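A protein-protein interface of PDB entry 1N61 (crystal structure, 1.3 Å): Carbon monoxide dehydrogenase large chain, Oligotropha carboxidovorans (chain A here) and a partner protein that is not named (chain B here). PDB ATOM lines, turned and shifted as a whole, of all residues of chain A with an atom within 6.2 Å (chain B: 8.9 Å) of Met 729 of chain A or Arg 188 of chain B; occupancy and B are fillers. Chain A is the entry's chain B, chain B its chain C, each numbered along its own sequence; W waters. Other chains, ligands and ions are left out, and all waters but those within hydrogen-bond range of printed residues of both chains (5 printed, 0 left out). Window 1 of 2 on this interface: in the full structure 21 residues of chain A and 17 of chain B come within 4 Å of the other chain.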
ATOM      1  N   ARG A 716      -3.079  -8.532  33.296  1.00  0.00           N
ATOM      2  CA  ARG A 716      -2.753  -7.113  33.412  1.00  0.00           C
ATOM      3  C   ARG A 716      -3.686  -6.461  34.416  1.00  0.00           C
ATOM      4  O   ARG A 716      -4.767  -6.989  34.731  1.00  0.00           O
ATOM      5  CB  ARG A 716      -2.917  -6.426  32.055  1.00  0.00           C
ATOM      6  CG  ARG A 716      -1.865  -6.754  30.986  1.00  0.00           C
ATOM      7  CD  ARG A 716      -2.081  -5.998  29.641  1.00  0.00           C
ATOM      8  NE  ARG A 716      -3.097  -6.638  28.795  1.00  0.00           N
ATOM      9  CZ  ARG A 716      -4.366  -6.227  28.658  1.00  0.00           C
ATOM     10  NH1 ARG A 716      -4.720  -5.007  29.035  1.00  0.00           N
ATOM     11  NH2 ARG A 716      -5.290  -7.041  28.139  1.00  0.00           N
ATOM     12  N   GLY A 725      -7.910  -9.208  31.028  1.00  0.00           N
ATOM     13  CA  GLY A 725      -7.563 -10.380  30.262  1.00  0.00           C
ATOM     14  C   GLY A 725      -7.599 -11.675  31.062  1.00  0.00           C
ATOM     15  O   GLY A 725      -7.164 -12.708  30.541  1.00  0.00           O
ATOM     16  N   SER A 727      -9.675 -14.089  31.459  1.00  0.00           N
ATOM     17  CA  SER A 727     -10.612 -15.125  31.001  1.00  0.00           C
ATOM     18  C   SER A 727     -10.072 -15.714  29.725  1.00  0.00           C
ATOM     19  O   SER A 727      -9.213 -15.103  29.090  1.00  0.00           O
ATOM     20  CB  SER A 727     -12.001 -14.563  30.736  1.00  0.00           C
ATOM     21  OG  SER A 727     -12.055 -13.920  29.463  1.00  0.00           O
ATOM     22  N   PHE A 728     -10.621 -16.839  29.280  1.00  0.00           N
ATOM     23  CA  PHE A 728     -10.158 -17.419  28.048  1.00  0.00           C
ATOM     24  C   PHE A 728     -10.591 -16.624  26.807  1.00  0.00           C
ATOM     25  O   PHE A 728     -10.204 -16.964  25.687  1.00  0.00           O
ATOM     26  CB  PHE A 728     -10.529 -18.894  27.944  1.00  0.00           C
ATOM     27  CG  PHE A 728      -9.819 -19.807  28.915  1.00  0.00           C
ATOM     28  CD1 PHE A 728      -8.695 -19.413  29.636  1.00  0.00           C
ATOM     29  CD2 PHE A 728     -10.275 -21.116  29.069  1.00  0.00           C
ATOM     30  CE1 PHE A 728      -8.098 -20.285  30.518  1.00  0.00           C
ATOM     31  CE2 PHE A 728      -9.623 -22.006  29.915  1.00  0.00           C
ATOM     32  CZ  PHE A 728      -8.537 -21.583  30.626  1.00  0.00           C
ATOM     33  N   MET A 729     -11.337 -15.532  26.967  1.00  0.00           N
ATOM     34  CA  MET A 729     -11.521 -14.589  25.838  1.00  0.00           C
ATOM     35  C   MET A 729     -10.191 -13.972  25.383  1.00  0.00           C
ATOM     36  O   MET A 729     -10.075 -13.591  24.221  1.00  0.00           O
ATOM     37  CB  MET A 729     -12.479 -13.491  26.240  1.00  0.00           C
ATOM     38  CG  MET A 729     -13.886 -13.966  26.524  1.00  0.00           C
ATOM     39  SD  MET A 729     -14.910 -14.335  25.204  1.00  0.00           S
ATOM     40  CE  MET A 729     -14.323 -13.725  24.100  1.00  0.00           C
ATOM     41  N   ASP A 730      -9.251 -13.778  26.310  1.00  0.00           N
ATOM     42  CA  ASP A 730      -8.017 -13.026  26.045  1.00  0.00           C
ATOM     43  C   ASP A 730      -6.771 -13.754  26.470  1.00  0.00           C
ATOM     44  O   ASP A 730      -5.741 -13.571  25.861  1.00  0.00           O
ATOM     45  CB  ASP A 730      -8.043 -11.685  26.766  1.00  0.00           C
ATOM     46  CG  ASP A 730      -9.142 -10.824  26.262  1.00  0.00           C
ATOM     47  OD1 ASP A 730      -8.964 -10.234  25.164  1.00  0.00           O
ATOM     48  OD2 ASP A 730     -10.157 -10.604  26.957  1.00  0.00           O
ATOM     49  N   PHE A 731      -6.898 -14.594  27.472  1.00  0.00           N
ATOM     50  CA  PHE A 731      -5.682 -15.208  28.076  1.00  0.00           C
ATOM     51  C   PHE A 731      -5.188 -16.285  27.093  1.00  0.00           C
ATOM     52  O   PHE A 731      -5.926 -17.217  26.809  1.00  0.00           O
ATOM     53  CB  PHE A 731      -6.059 -15.872  29.396  1.00  0.00           C
ATOM     54  CG  PHE A 731      -4.883 -16.490  30.135  1.00  0.00           C
ATOM     55  CD1 PHE A 731      -3.975 -15.693  30.834  1.00  0.00           C
ATOM     56  CD2 PHE A 731      -4.730 -17.866  30.189  1.00  0.00           C
ATOM     57  CE1 PHE A 731      -2.977 -16.286  31.577  1.00  0.00           C
ATOM     58  CE2 PHE A 731      -3.682 -18.426  30.883  1.00  0.00           C
ATOM     59  CZ  PHE A 731      -2.798 -17.614  31.534  1.00  0.00           C
ATOM     60  N   PHE A 732      -3.990 -16.130  26.570  1.00  0.00           N
ATOM     61  CA  PHE A 732      -3.521 -16.938  25.448  1.00  0.00           C
ATOM     62  C   PHE A 732      -3.159 -18.372  25.878  1.00  0.00           C
ATOM     63  O   PHE A 732      -2.100 -18.636  26.363  1.00  0.00           O
ATOM     64  CB  PHE A 732      -2.307 -16.280  24.801  1.00  0.00           C
ATOM     65  CG  PHE A 732      -1.786 -17.012  23.599  1.00  0.00           C
ATOM     66  CD1 PHE A 732      -2.538 -17.117  22.440  1.00  0.00           C
ATOM     67  CD2 PHE A 732      -0.512 -17.538  23.614  1.00  0.00           C
ATOM     68  CE1 PHE A 732      -2.016 -17.693  21.306  1.00  0.00           C
ATOM     69  CE2 PHE A 732      -0.001 -18.130  22.444  1.00  0.00           C
ATOM     70  CZ  PHE A 732      -0.783 -18.247  21.328  1.00  0.00           C
ATOM     71  N   GLU A 738      -2.066 -23.455  16.977  1.00  0.00           N
ATOM     72  CA  GLU A 738      -0.977 -22.543  17.251  1.00  0.00           C
ATOM     73  C   GLU A 738       0.289 -23.263  17.746  1.00  0.00           C
ATOM     74  O   GLU A 738       1.380 -22.701  17.648  1.00  0.00           O
ATOM     75  CB  GLU A 738      -1.372 -21.500  18.288  1.00  0.00           C
ATOM     76  CG  GLU A 738      -2.458 -20.527  17.821  1.00  0.00           C
ATOM     77  CD  GLU A 738      -3.843 -21.132  17.867  1.00  0.00           C
ATOM     78  OE1 GLU A 738      -4.097 -21.944  18.798  1.00  0.00           O
ATOM     79  OE2 GLU A 738      -4.692 -20.681  17.096  1.00  0.00           O
ATOM     80  N   ASP A 794       3.490 -10.783  21.211  1.00  0.00           N
ATOM     81  CA  ASP A 794       2.300 -10.947  20.398  1.00  0.00           C
ATOM     82  C   ASP A 794       2.314  -9.931  19.294  1.00  0.00           C
ATOM     83  O   ASP A 794       3.201  -9.085  19.206  1.00  0.00           O
ATOM     84  CB  ASP A 794       1.011 -10.928  21.195  1.00  0.00           C
ATOM     85  CG  ASP A 794       0.746  -9.671  21.900  1.00  0.00           C
ATOM     86  OD1 ASP A 794       1.572  -8.718  21.838  1.00  0.00           O
ATOM     87  OD2 ASP A 794      -0.282  -9.543  22.634  1.00  0.00           O
ATOM     88  N   HIS B  35     -24.805 -19.762  21.235  1.00  0.00           N
ATOM     89  CA  HIS B  35     -23.371 -19.631  21.486  1.00  0.00           C
ATOM     90  C   HIS B  35     -22.863 -18.200  21.630  1.00  0.00           C
ATOM     91  O   HIS B  35     -21.690 -17.984  21.866  1.00  0.00           O
ATOM     92  CB  HIS B  35     -22.507 -20.544  20.578  1.00  0.00           C
ATOM     93  CG  HIS B  35     -22.558 -21.970  20.963  1.00  0.00           C
ATOM     94  ND1 HIS B  35     -23.752 -22.669  21.101  1.00  0.00           N
ATOM     95  CD2 HIS B  35     -21.573 -22.838  21.284  1.00  0.00           C
ATOM     96  CE1 HIS B  35     -23.480 -23.888  21.562  1.00  0.00           C
ATOM     97  NE2 HIS B  35     -22.175 -24.016  21.688  1.00  0.00           N
ATOM     98  N   PRO B  39     -23.523 -17.794  26.776  1.00  0.00           N
ATOM     99  CA  PRO B  39     -22.357 -17.264  27.478  1.00  0.00           C
ATOM    100  C   PRO B  39     -22.619 -15.982  28.260  1.00  0.00           C
ATOM    101  O   PRO B  39     -22.164 -15.855  29.391  1.00  0.00           O
ATOM    102  CB  PRO B  39     -21.322 -17.108  26.388  1.00  0.00           C
ATOM    103  CG  PRO B  39     -21.676 -18.245  25.428  1.00  0.00           C
ATOM    104  CD  PRO B  39     -23.180 -18.266  25.415  1.00  0.00           C
ATOM    105  N   ILE B  40     -23.426 -15.059  27.726  1.00  0.00           N
ATOM    106  CA  ILE B  40     -23.695 -13.880  28.493  1.00  0.00           C
ATOM    107  C   ILE B  40     -24.768 -14.023  29.552  1.00  0.00           C
ATOM    108  O   ILE B  40     -24.814 -13.253  30.494  1.00  0.00           O
ATOM    109  CB  ILE B  40     -23.959 -12.657  27.628  1.00  0.00           C
ATOM    110  CG1 ILE B  40     -25.182 -12.837  26.751  1.00  0.00           C
ATOM    111  CG2 ILE B  40     -22.689 -12.291  26.861  1.00  0.00           C
ATOM    112  CD1 ILE B  40     -25.507 -11.584  26.079  1.00  0.00           C
ATOM    113  N   THR B  43     -22.719 -15.236  32.621  1.00  0.00           N
ATOM    114  CA  THR B  43     -22.053 -14.165  33.370  1.00  0.00           C
ATOM    115  C   THR B  43     -23.050 -13.173  34.002  1.00  0.00           C
ATOM    116  O   THR B  43     -22.629 -12.226  34.676  1.00  0.00           O
ATOM    117  CB  THR B  43     -21.123 -13.355  32.482  1.00  0.00           C
ATOM    118  OG1 THR B  43     -21.886 -12.770  31.423  1.00  0.00           O
ATOM    119  CG2 THR B  43     -20.083 -14.235  31.820  1.00  0.00           C
ATOM    120  N   ASP B 120     -22.781  -8.033  17.935  1.00  0.00           N
ATOM    121  CA  ASP B 120     -21.417  -7.915  18.418  1.00  0.00           C
ATOM    122  C   ASP B 120     -20.578  -7.532  17.215  1.00  0.00           C
ATOM    123  O   ASP B 120     -20.586  -8.239  16.237  1.00  0.00           O
ATOM    124  CB  ASP B 120     -21.030  -9.296  18.922  1.00  0.00           C
ATOM    125  CG  ASP B 120     -19.697  -9.351  19.593  1.00  0.00           C
ATOM    126  OD1 ASP B 120     -18.842  -8.456  19.411  1.00  0.00           O
ATOM    127  OD2 ASP B 120     -19.490 -10.272  20.417  1.00  0.00           O
ATOM    128  N   LYS B 185      -8.617 -12.746   7.802  1.00  0.00           N
ATOM    129  CA  LYS B 185      -8.816 -12.431   9.193  1.00  0.00           C
ATOM    130  C   LYS B 185      -7.478 -12.477   9.928  1.00  0.00           C
ATOM    131  O   LYS B 185      -6.791 -13.481   9.845  1.00  0.00           O
ATOM    132  CB  LYS B 185      -9.844 -13.435   9.759  1.00  0.00           C
ATOM    133  CG  LYS B 185     -10.228 -13.237  11.200  1.00  0.00           C
ATOM    134  CD  LYS B 185     -11.334 -14.161  11.690  1.00  0.00           C
ATOM    135  CE  LYS B 185     -11.693 -14.042  13.141  1.00  0.00           C
ATOM    136  NZ  LYS B 185     -12.937 -14.853  13.488  1.00  0.00           N
ATOM    137  N   LEU B 186      -7.233 -11.499  10.793  1.00  0.00           N
ATOM    138  CA  LEU B 186      -6.125 -11.460  11.725  1.00  0.00           C
ATOM    139  C   LEU B 186      -6.663 -11.675  13.109  1.00  0.00           C
ATOM    140  O   LEU B 186      -7.569 -10.968  13.501  1.00  0.00           O
ATOM    141  CB  LEU B 186      -5.431 -10.095  11.666  1.00  0.00           C
ATOM    142  CG  LEU B 186      -4.223  -9.949  12.570  1.00  0.00           C
ATOM    143  CD1 LEU B 186      -3.176 -10.989  12.289  1.00  0.00           C
ATOM    144  CD2 LEU B 186      -3.628  -8.592  12.468  1.00  0.00           C
ATOM    145  N   LYS B 187      -6.205 -12.686  13.826  1.00  0.00           N
ATOM    146  CA  LYS B 187      -6.726 -12.990  15.136  1.00  0.00           C
ATOM    147  C   LYS B 187      -5.618 -13.576  16.022  1.00  0.00           C
ATOM    148  O   LYS B 187      -4.587 -14.001  15.538  1.00  0.00           O
ATOM    149  CB  LYS B 187      -7.896 -13.988  15.029  1.00  0.00           C
ATOM    150  CG  LYS B 187      -7.491 -15.309  14.465  1.00  0.00           C
ATOM    151  CD  LYS B 187      -8.730 -16.174  14.157  1.00  0.00           C
ATOM    152  CE  LYS B 187      -8.429 -17.624  13.836  1.00  0.00           C
ATOM    153  NZ  LYS B 187      -7.502 -17.788  12.712  1.00  0.00           N
ATOM    154  N   ARG B 188      -5.836 -13.592  17.321  1.00  0.00           N
ATOM    155  CA  ARG B 188      -4.782 -14.032  18.240  1.00  0.00           C
ATOM    156  C   ARG B 188      -4.647 -15.560  18.320  1.00  0.00           C
ATOM    157  O   ARG B 188      -3.576 -16.055  18.624  1.00  0.00           O
ATOM    158  CB  ARG B 188      -5.079 -13.481  19.642  1.00  0.00           C
ATOM    159  CG  ARG B 188      -4.839 -11.968  19.791  1.00  0.00           C
ATOM    160  CD  ARG B 188      -5.318 -11.389  21.115  1.00  0.00           C
ATOM    161  NE  ARG B 188      -6.747 -11.606  21.306  1.00  0.00           N
ATOM    162  CZ  ARG B 188      -7.416 -11.193  22.352  1.00  0.00           C
ATOM    163  NH1 ARG B 188      -6.772 -10.623  23.389  1.00  0.00           N
ATOM    164  NH2 ARG B 188      -8.739 -11.320  22.368  1.00  0.00           N
ATOM    165  N   LYS B 189      -5.735 -16.279  18.037  1.00  0.00           N
ATOM    166  CA  LYS B 189      -5.764 -17.726  18.080  1.00  0.00           C
ATOM    167  C   LYS B 189      -7.103 -18.158  17.499  1.00  0.00           C
ATOM    168  O   LYS B 189      -8.030 -17.345  17.349  1.00  0.00           O
ATOM    169  CB  LYS B 189      -5.575 -18.250  19.523  1.00  0.00           C
ATOM    170  CG  LYS B 189      -6.514 -17.642  20.551  1.00  0.00           C
ATOM    171  CD  LYS B 189      -6.423 -18.284  21.926  1.00  0.00           C
ATOM    172  CE  LYS B 189      -7.331 -19.481  21.976  1.00  0.00           C
ATOM    173  NZ  LYS B 189      -7.298 -20.167  23.324  1.00  0.00           N
ATOM    174  N   ILE B 190      -7.238 -19.457  17.240  1.00  0.00           N
ATOM    175  CA  ILE B 190      -8.515 -20.062  16.885  1.00  0.00           C
ATOM    176  C   ILE B 190      -9.558 -19.544  17.848  1.00  0.00           C
ATOM    177  O   ILE B 190      -9.414 -19.622  19.058  1.00  0.00           O
ATOM    178  CB  ILE B 190      -8.388 -21.606  17.025  1.00  0.00           C
ATOM    179  CG1 ILE B 190      -7.534 -22.212  15.934  1.00  0.00           C
ATOM    180  CG2 ILE B 190      -9.767 -22.263  17.100  1.00  0.00           C
ATOM    181  CD1 ILE B 190      -8.033 -21.913  14.519  1.00  0.00           C
ATOM    182  N   GLY B 191     -10.724 -19.162  17.304  1.00  0.00           N
ATOM    183  CA  GLY B 191     -11.847 -18.793  18.120  1.00  0.00           C
ATOM    184  C   GLY B 191     -11.920 -17.335  18.477  1.00  0.00           C
ATOM    185  O   GLY B 191     -12.962 -16.860  18.912  1.00  0.00           O
ATOM    186  N   ASP B 192     -10.830 -16.605  18.295  1.00  0.00           N
ATOM    187  CA  ASP B 192     -10.807 -15.209  18.722  1.00  0.00           C
ATOM    188  C   ASP B 192     -11.492 -14.337  17.655  1.00  0.00           C
ATOM    189  O   ASP B 192     -11.411 -14.613  16.456  1.00  0.00           O
ATOM    190  CB  ASP B 192      -9.372 -14.829  18.893  1.00  0.00           C
ATOM    191  CG  ASP B 192      -9.139 -13.431  19.411  1.00  0.00           C
ATOM    192  OD1 ASP B 192      -9.980 -12.960  20.206  1.00  0.00           O
ATOM    193  OD2 ASP B 192      -8.079 -12.789  19.118  1.00  0.00           O
ATOM    194  N   TYR B 193     -12.233 -13.331  18.085  1.00  0.00           N
ATOM    195  CA  TYR B 193     -12.776 -12.330  17.192  1.00  0.00           C
ATOM    196  C   TYR B 193     -11.600 -11.559  16.584  1.00  0.00           C
ATOM    197  O   TYR B 193     -10.513 -11.413  17.201  1.00  0.00           O
ATOM    198  CB  TYR B 193     -13.711 -11.401  17.982  1.00  0.00           C
ATOM    199  CG  TYR B 193     -14.819 -12.150  18.651  1.00  0.00           C
ATOM    200  CD1 TYR B 193     -15.907 -12.608  17.939  1.00  0.00           C
ATOM    201  CD2 TYR B 193     -14.748 -12.480  20.006  1.00  0.00           C
ATOM    202  CE1 TYR B 193     -16.952 -13.284  18.585  1.00  0.00           C
ATOM    203  CE2 TYR B 193     -15.767 -13.175  20.661  1.00  0.00           C
ATOM    204  CZ  TYR B 193     -16.824 -13.671  19.929  1.00  0.00           C
ATOM    205  OH  TYR B 193     -17.827 -14.409  20.542  1.00  0.00           O
ATOM    206  N   ALA B 194     -11.832 -11.002  15.413  1.00  0.00           N
ATOM    207  CA  ALA B 194     -10.718 -10.457  14.604  1.00  0.00           C
ATOM    208  C   ALA B 194     -10.110  -9.206  15.243  1.00  0.00           C
ATOM    209  O   ALA B 194     -10.829  -8.336  15.745  1.00  0.00           O
ATOM    210  CB  ALA B 194     -11.244 -10.076  13.244  1.00  0.00           C
ATOM    211  N   THR B 195      -8.806  -9.149  15.267  1.00  0.00           N
ATOM    212  CA  THR B 195      -8.113  -7.878  15.360  1.00  0.00           C
ATOM    213  C   THR B 195      -8.568  -6.962  14.246  1.00  0.00           C
ATOM    214  O   THR B 195      -8.864  -5.772  14.479  1.00  0.00           O
ATOM    215  CB  THR B 195      -6.622  -8.172  15.322  1.00  0.00           C
ATOM    216  OG1 THR B 195      -6.284  -9.067  16.421  1.00  0.00           O
ATOM    217  CG2 THR B 195      -5.781  -6.915  15.393  1.00  0.00           C
ATOM    218  N   ALA B 196      -8.664  -7.541  13.042  1.00  0.00           N
ATOM    219  CA  ALA B 196      -9.274  -6.906  11.863  1.00  0.00           C
ATOM    220  C   ALA B 196      -9.502  -8.001  10.875  1.00  0.00           C
ATOM    221  O   ALA B 196      -8.756  -8.978  10.863  1.00  0.00           O
ATOM    222  CB  ALA B 196      -8.366  -5.857  11.298  1.00  0.00           C
ATOM    223  N   ASN B 218     -14.930  -5.897  12.745  1.00  0.00           N
ATOM    224  CA  ASN B 218     -14.446  -5.658  14.093  1.00  0.00           C
ATOM    225  C   ASN B 218     -13.406  -4.528  14.166  1.00  0.00           C
ATOM    226  O   ASN B 218     -12.519  -4.543  15.034  1.00  0.00           O
ATOM    227  CB  ASN B 218     -13.906  -6.926  14.784  1.00  0.00           C
ATOM    228  CG  ASN B 218     -14.050  -6.881  16.300  1.00  0.00           C
ATOM    229  OD1 ASN B 218     -14.896  -6.166  16.811  1.00  0.00           O
ATOM    230  ND2 ASN B 218     -13.248  -7.700  17.020  1.00  0.00           N
ATOM    231  N   ASP B 259      -8.235  -2.831  22.913  1.00  0.00           N
ATOM    232  CA  ASP B 259      -8.410  -3.887  23.904  1.00  0.00           C
ATOM    233  C   ASP B 259      -7.200  -4.835  23.845  1.00  0.00           C
ATOM    234  O   ASP B 259      -6.142  -4.437  23.399  1.00  0.00           O
ATOM    235  CB  ASP B 259      -9.798  -4.581  23.695  1.00  0.00           C
ATOM    236  CG  ASP B 259      -9.982  -5.182  22.301  1.00  0.00           C
ATOM    237  OD1 ASP B 259      -9.032  -5.771  21.757  1.00  0.00           O
ATOM    238  OD2 ASP B 259     -11.111  -5.278  21.771  1.00  0.00           O
ATOM    239  N   GLY B 260      -7.346  -6.068  24.267  1.00  0.00           N
ATOM    240  CA  GLY B 260      -6.253  -7.011  24.274  1.00  0.00           C
ATOM    241  C   GLY B 260      -5.680  -7.344  22.900  1.00  0.00           C
ATOM    242  O   GLY B 260      -4.564  -7.878  22.804  1.00  0.00           O
ATOM    243  N   ARG B 261      -6.408  -7.007  21.839  1.00  0.00           N
ATOM    244  CA  ARG B 261      -5.905  -7.203  20.494  1.00  0.00           C
ATOM    245  C   ARG B 261      -4.935  -6.113  20.046  1.00  0.00           C
ATOM    246  O   ARG B 261      -4.343  -6.180  18.973  1.00  0.00           O
ATOM    247  CB  ARG B 261      -7.105  -7.258  19.567  1.00  0.00           C
ATOM    248  CG  ARG B 261      -7.993  -8.474  19.848  1.00  0.00           C
ATOM    249  CD  ARG B 261      -9.297  -8.531  19.089  1.00  0.00           C
ATOM    250  NE  ARG B 261     -10.159  -9.614  19.524  1.00  0.00           N
ATOM    251  CZ  ARG B 261     -10.912  -9.567  20.613  1.00  0.00           C
ATOM    252  NH1 ARG B 261     -10.981  -8.461  21.351  1.00  0.00           N
ATOM    253  NH2 ARG B 261     -11.557 -10.648  20.965  1.00  0.00           N
ATOM    254  N   GLY B 262      -4.863  -5.038  20.804  1.00  0.00           N
ATOM    255  CA  GLY B 262      -3.951  -3.968  20.510  1.00  0.00           C
ATOM    256  C   GLY B 262      -4.637  -2.616  20.539  1.00  0.00           C
ATOM    257  O   GLY B 262      -5.844  -2.516  20.594  1.00  0.00           O
ATOM    258  N   TYR B 266      -3.238   0.353  15.656  1.00  0.00           N
ATOM    259  CA  TYR B 266      -2.796  -0.927  15.125  1.00  0.00           C
ATOM    260  C   TYR B 266      -3.914  -1.603  14.348  1.00  0.00           C
ATOM    261  O   TYR B 266      -3.735  -2.094  13.231  1.00  0.00           O
ATOM    262  CB  TYR B 266      -2.249  -1.849  16.229  1.00  0.00           C
ATOM    263  CG  TYR B 266      -2.011  -3.264  15.752  1.00  0.00           C
ATOM    264  CD1 TYR B 266      -1.022  -3.543  14.841  1.00  0.00           C
ATOM    265  CD2 TYR B 266      -2.681  -4.327  16.322  1.00  0.00           C
ATOM    266  CE1 TYR B 266      -0.731  -4.875  14.462  1.00  0.00           C
ATOM    267  CE2 TYR B 266      -2.382  -5.633  15.968  1.00  0.00           C
ATOM    268  CZ  TYR B 266      -1.387  -5.893  15.064  1.00  0.00           C
ATOM    269  OH  TYR B 266      -1.135  -7.191  14.661  1.00  0.00           O
ATOM    270  N   ARG B 267      -5.084  -1.624  14.939  1.00  0.00           N
ATOM    271  CA  ARG B 267      -6.225  -2.285  14.300  1.00  0.00           C
ATOM    272  C   ARG B 267      -6.675  -1.591  13.037  1.00  0.00           C
ATOM    273  O   ARG B 267      -7.009  -2.262  12.097  1.00  0.00           O
ATOM    274  CB  ARG B 267      -7.352  -2.413  15.288  1.00  0.00           C
ATOM    275  CG  ARG B 267      -6.884  -3.313  16.453  1.00  0.00           C
ATOM    276  CD  ARG B 267      -7.878  -3.536  17.493  1.00  0.00           C
ATOM    277  NE  ARG B 267      -8.945  -4.405  17.007  1.00  0.00           N
ATOM    278  CZ  ARG B 267      -9.908  -4.838  17.778  1.00  0.00           C
ATOM    279  NH1 ARG B 267     -10.074  -4.276  18.942  1.00  0.00           N
ATOM    280  NH2 ARG B 267     -10.798  -5.716  17.327  1.00  0.00           N
HETATM  281  O   HOH W   1      -2.712  -9.457  21.364  1.00  0.00           O
HETATM  282  O   HOH W   2      -7.890 -18.563  25.527  1.00  0.00           O
HETATM  283  O   HOH W   3     -16.494 -15.989  22.401  1.00  0.00           O
HETATM  284  O   HOH W   4     -11.953 -13.717  22.233  1.00  0.00           O
HETATM  285  O   HOH W   5      -9.624  -7.613  25.154  1.00  0.00           O
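OE2 of Glu 738 of chain A lies within hydrogen-bond range of N of Ile 190 of chain B (2.8 Å).
The guanidinium group of Arg 188 of chain B sits at hydrogen-bond distance from the backbone carbonyl oxygen of Met 729 of chain A (3.2 Å).
NH1 of Arg 188 of chain B is in salt-bridge range of OD1 of Asp 730 of chain A.
Water W5 bridges OD1 of Asp 730 of chain A (2.7 Å) and N of Gly 260 of chain B (2.9 Å).
Water W2 lies within hydrogen-bond range of O of Phe 731 of chain A (2.7 Å), NZ of Lys 189 of chain B (2.8 Å) and O of Phe 728 of chain A (2.8 Å).
Water W4 lies within hydrogen-bond range of the backbone carbonyl oxygen (O) of Met 729 of chain A (2.7 Å), the side-chain carboxylate (OD1) of Asp 192 of chain B (2.9 Å) and the guanidinium group (NH2) of Arg 261 of chain B (3.3 Å).
Water W1 lies within hydrogen-bond range of the side-chain carboxylate of Asp 794 of chain A (2.7 Å) and the backbone carbonyl oxygen of Gly 260 of chain B (2.8 Å).
Water W3 lies within hydrogen-bond range of OH of Tyr 193 of chain B (2.8 Å) and SD of Met 729 of chain A (3.6 Å).
The guanidinium group (NE) of Arg 188 of chain B is in salt-bridge range of the side-chain carboxylate (OD2) of Asp 192 of chain B (2.8 Å).
The backbone carbonyl oxygen (O) of Tyr 193 of chain B sits at hydrogen-bond distance from the guanidinium group (NE) of Arg 261 of chain B (3.0 Å).
The side-chain hydroxyl (OG) of Ser 727 of chain A lies close to the backbone NH (N) of Met 729 of chain A, at 3.1 Å.
Among the printed residues, pairs that only touch across the chains: Arg 716 of chain A with Gly 260 of chain B (3.98 Å), Met 729 of chain A with Tyr 193 of chain B (3.8 Å), Phe 732 of chain A with Arg 188 of chain B (3.5 Å) and Glu 738 of chain A with Lys 189 of chain B (3.3 Å).
Of the 24 printed residues of chain B, 5 touch a printed residue of chain A.
Hydrophobic or aromatic side chains of chain B that line the printed part of chain A: Ile 190 and Tyr 193.
Of the 10 printed residues of chain A, 5 touch a printed residue of chain B.
Printed residues of chain A that touch a printed residue of chain B: Arg 716, Met 729, Asp 730, Phe 732 and Glu 738.
Hydrophobic or aromatic side chains of chain A within 4 Å of the printed part of chain B: Met 729 and Phe 732.
Among the printed residues, Asp or Glu carboxylates within 4 Å of a Lys or Arg side-chain nitrogen of the other chain: Asp 730 of chain A with Arg 188 of chain B.
Of chain B, only Arg 188 (3.2 Å) and Tyr 193 (3.8 Å) come within 4 Å of Met 729 of chain A.
Arg 188 of chain B touches just these residues of chain A: Met 729, Asp 730 and Phe 732.
Of the printed residues of chain B, Arg 716 of chain A touches Gly 260.
Printed residues of chain A within 4 Å of Ile 190 of chain B: Glu 738.
Pro 39 of chain B touches none of the printed residues of chain A.
Gly 191 of chain B touches none of the printed residues of chain A.
The nearest residue of chain A that does not touch Arg 188 of chain B is Glu 738 of chain A (4.7 Å).
The nearest printed residue of chain B that does not touch Glu 738 of chain A is Arg 188 of chain B (4.7 Å).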
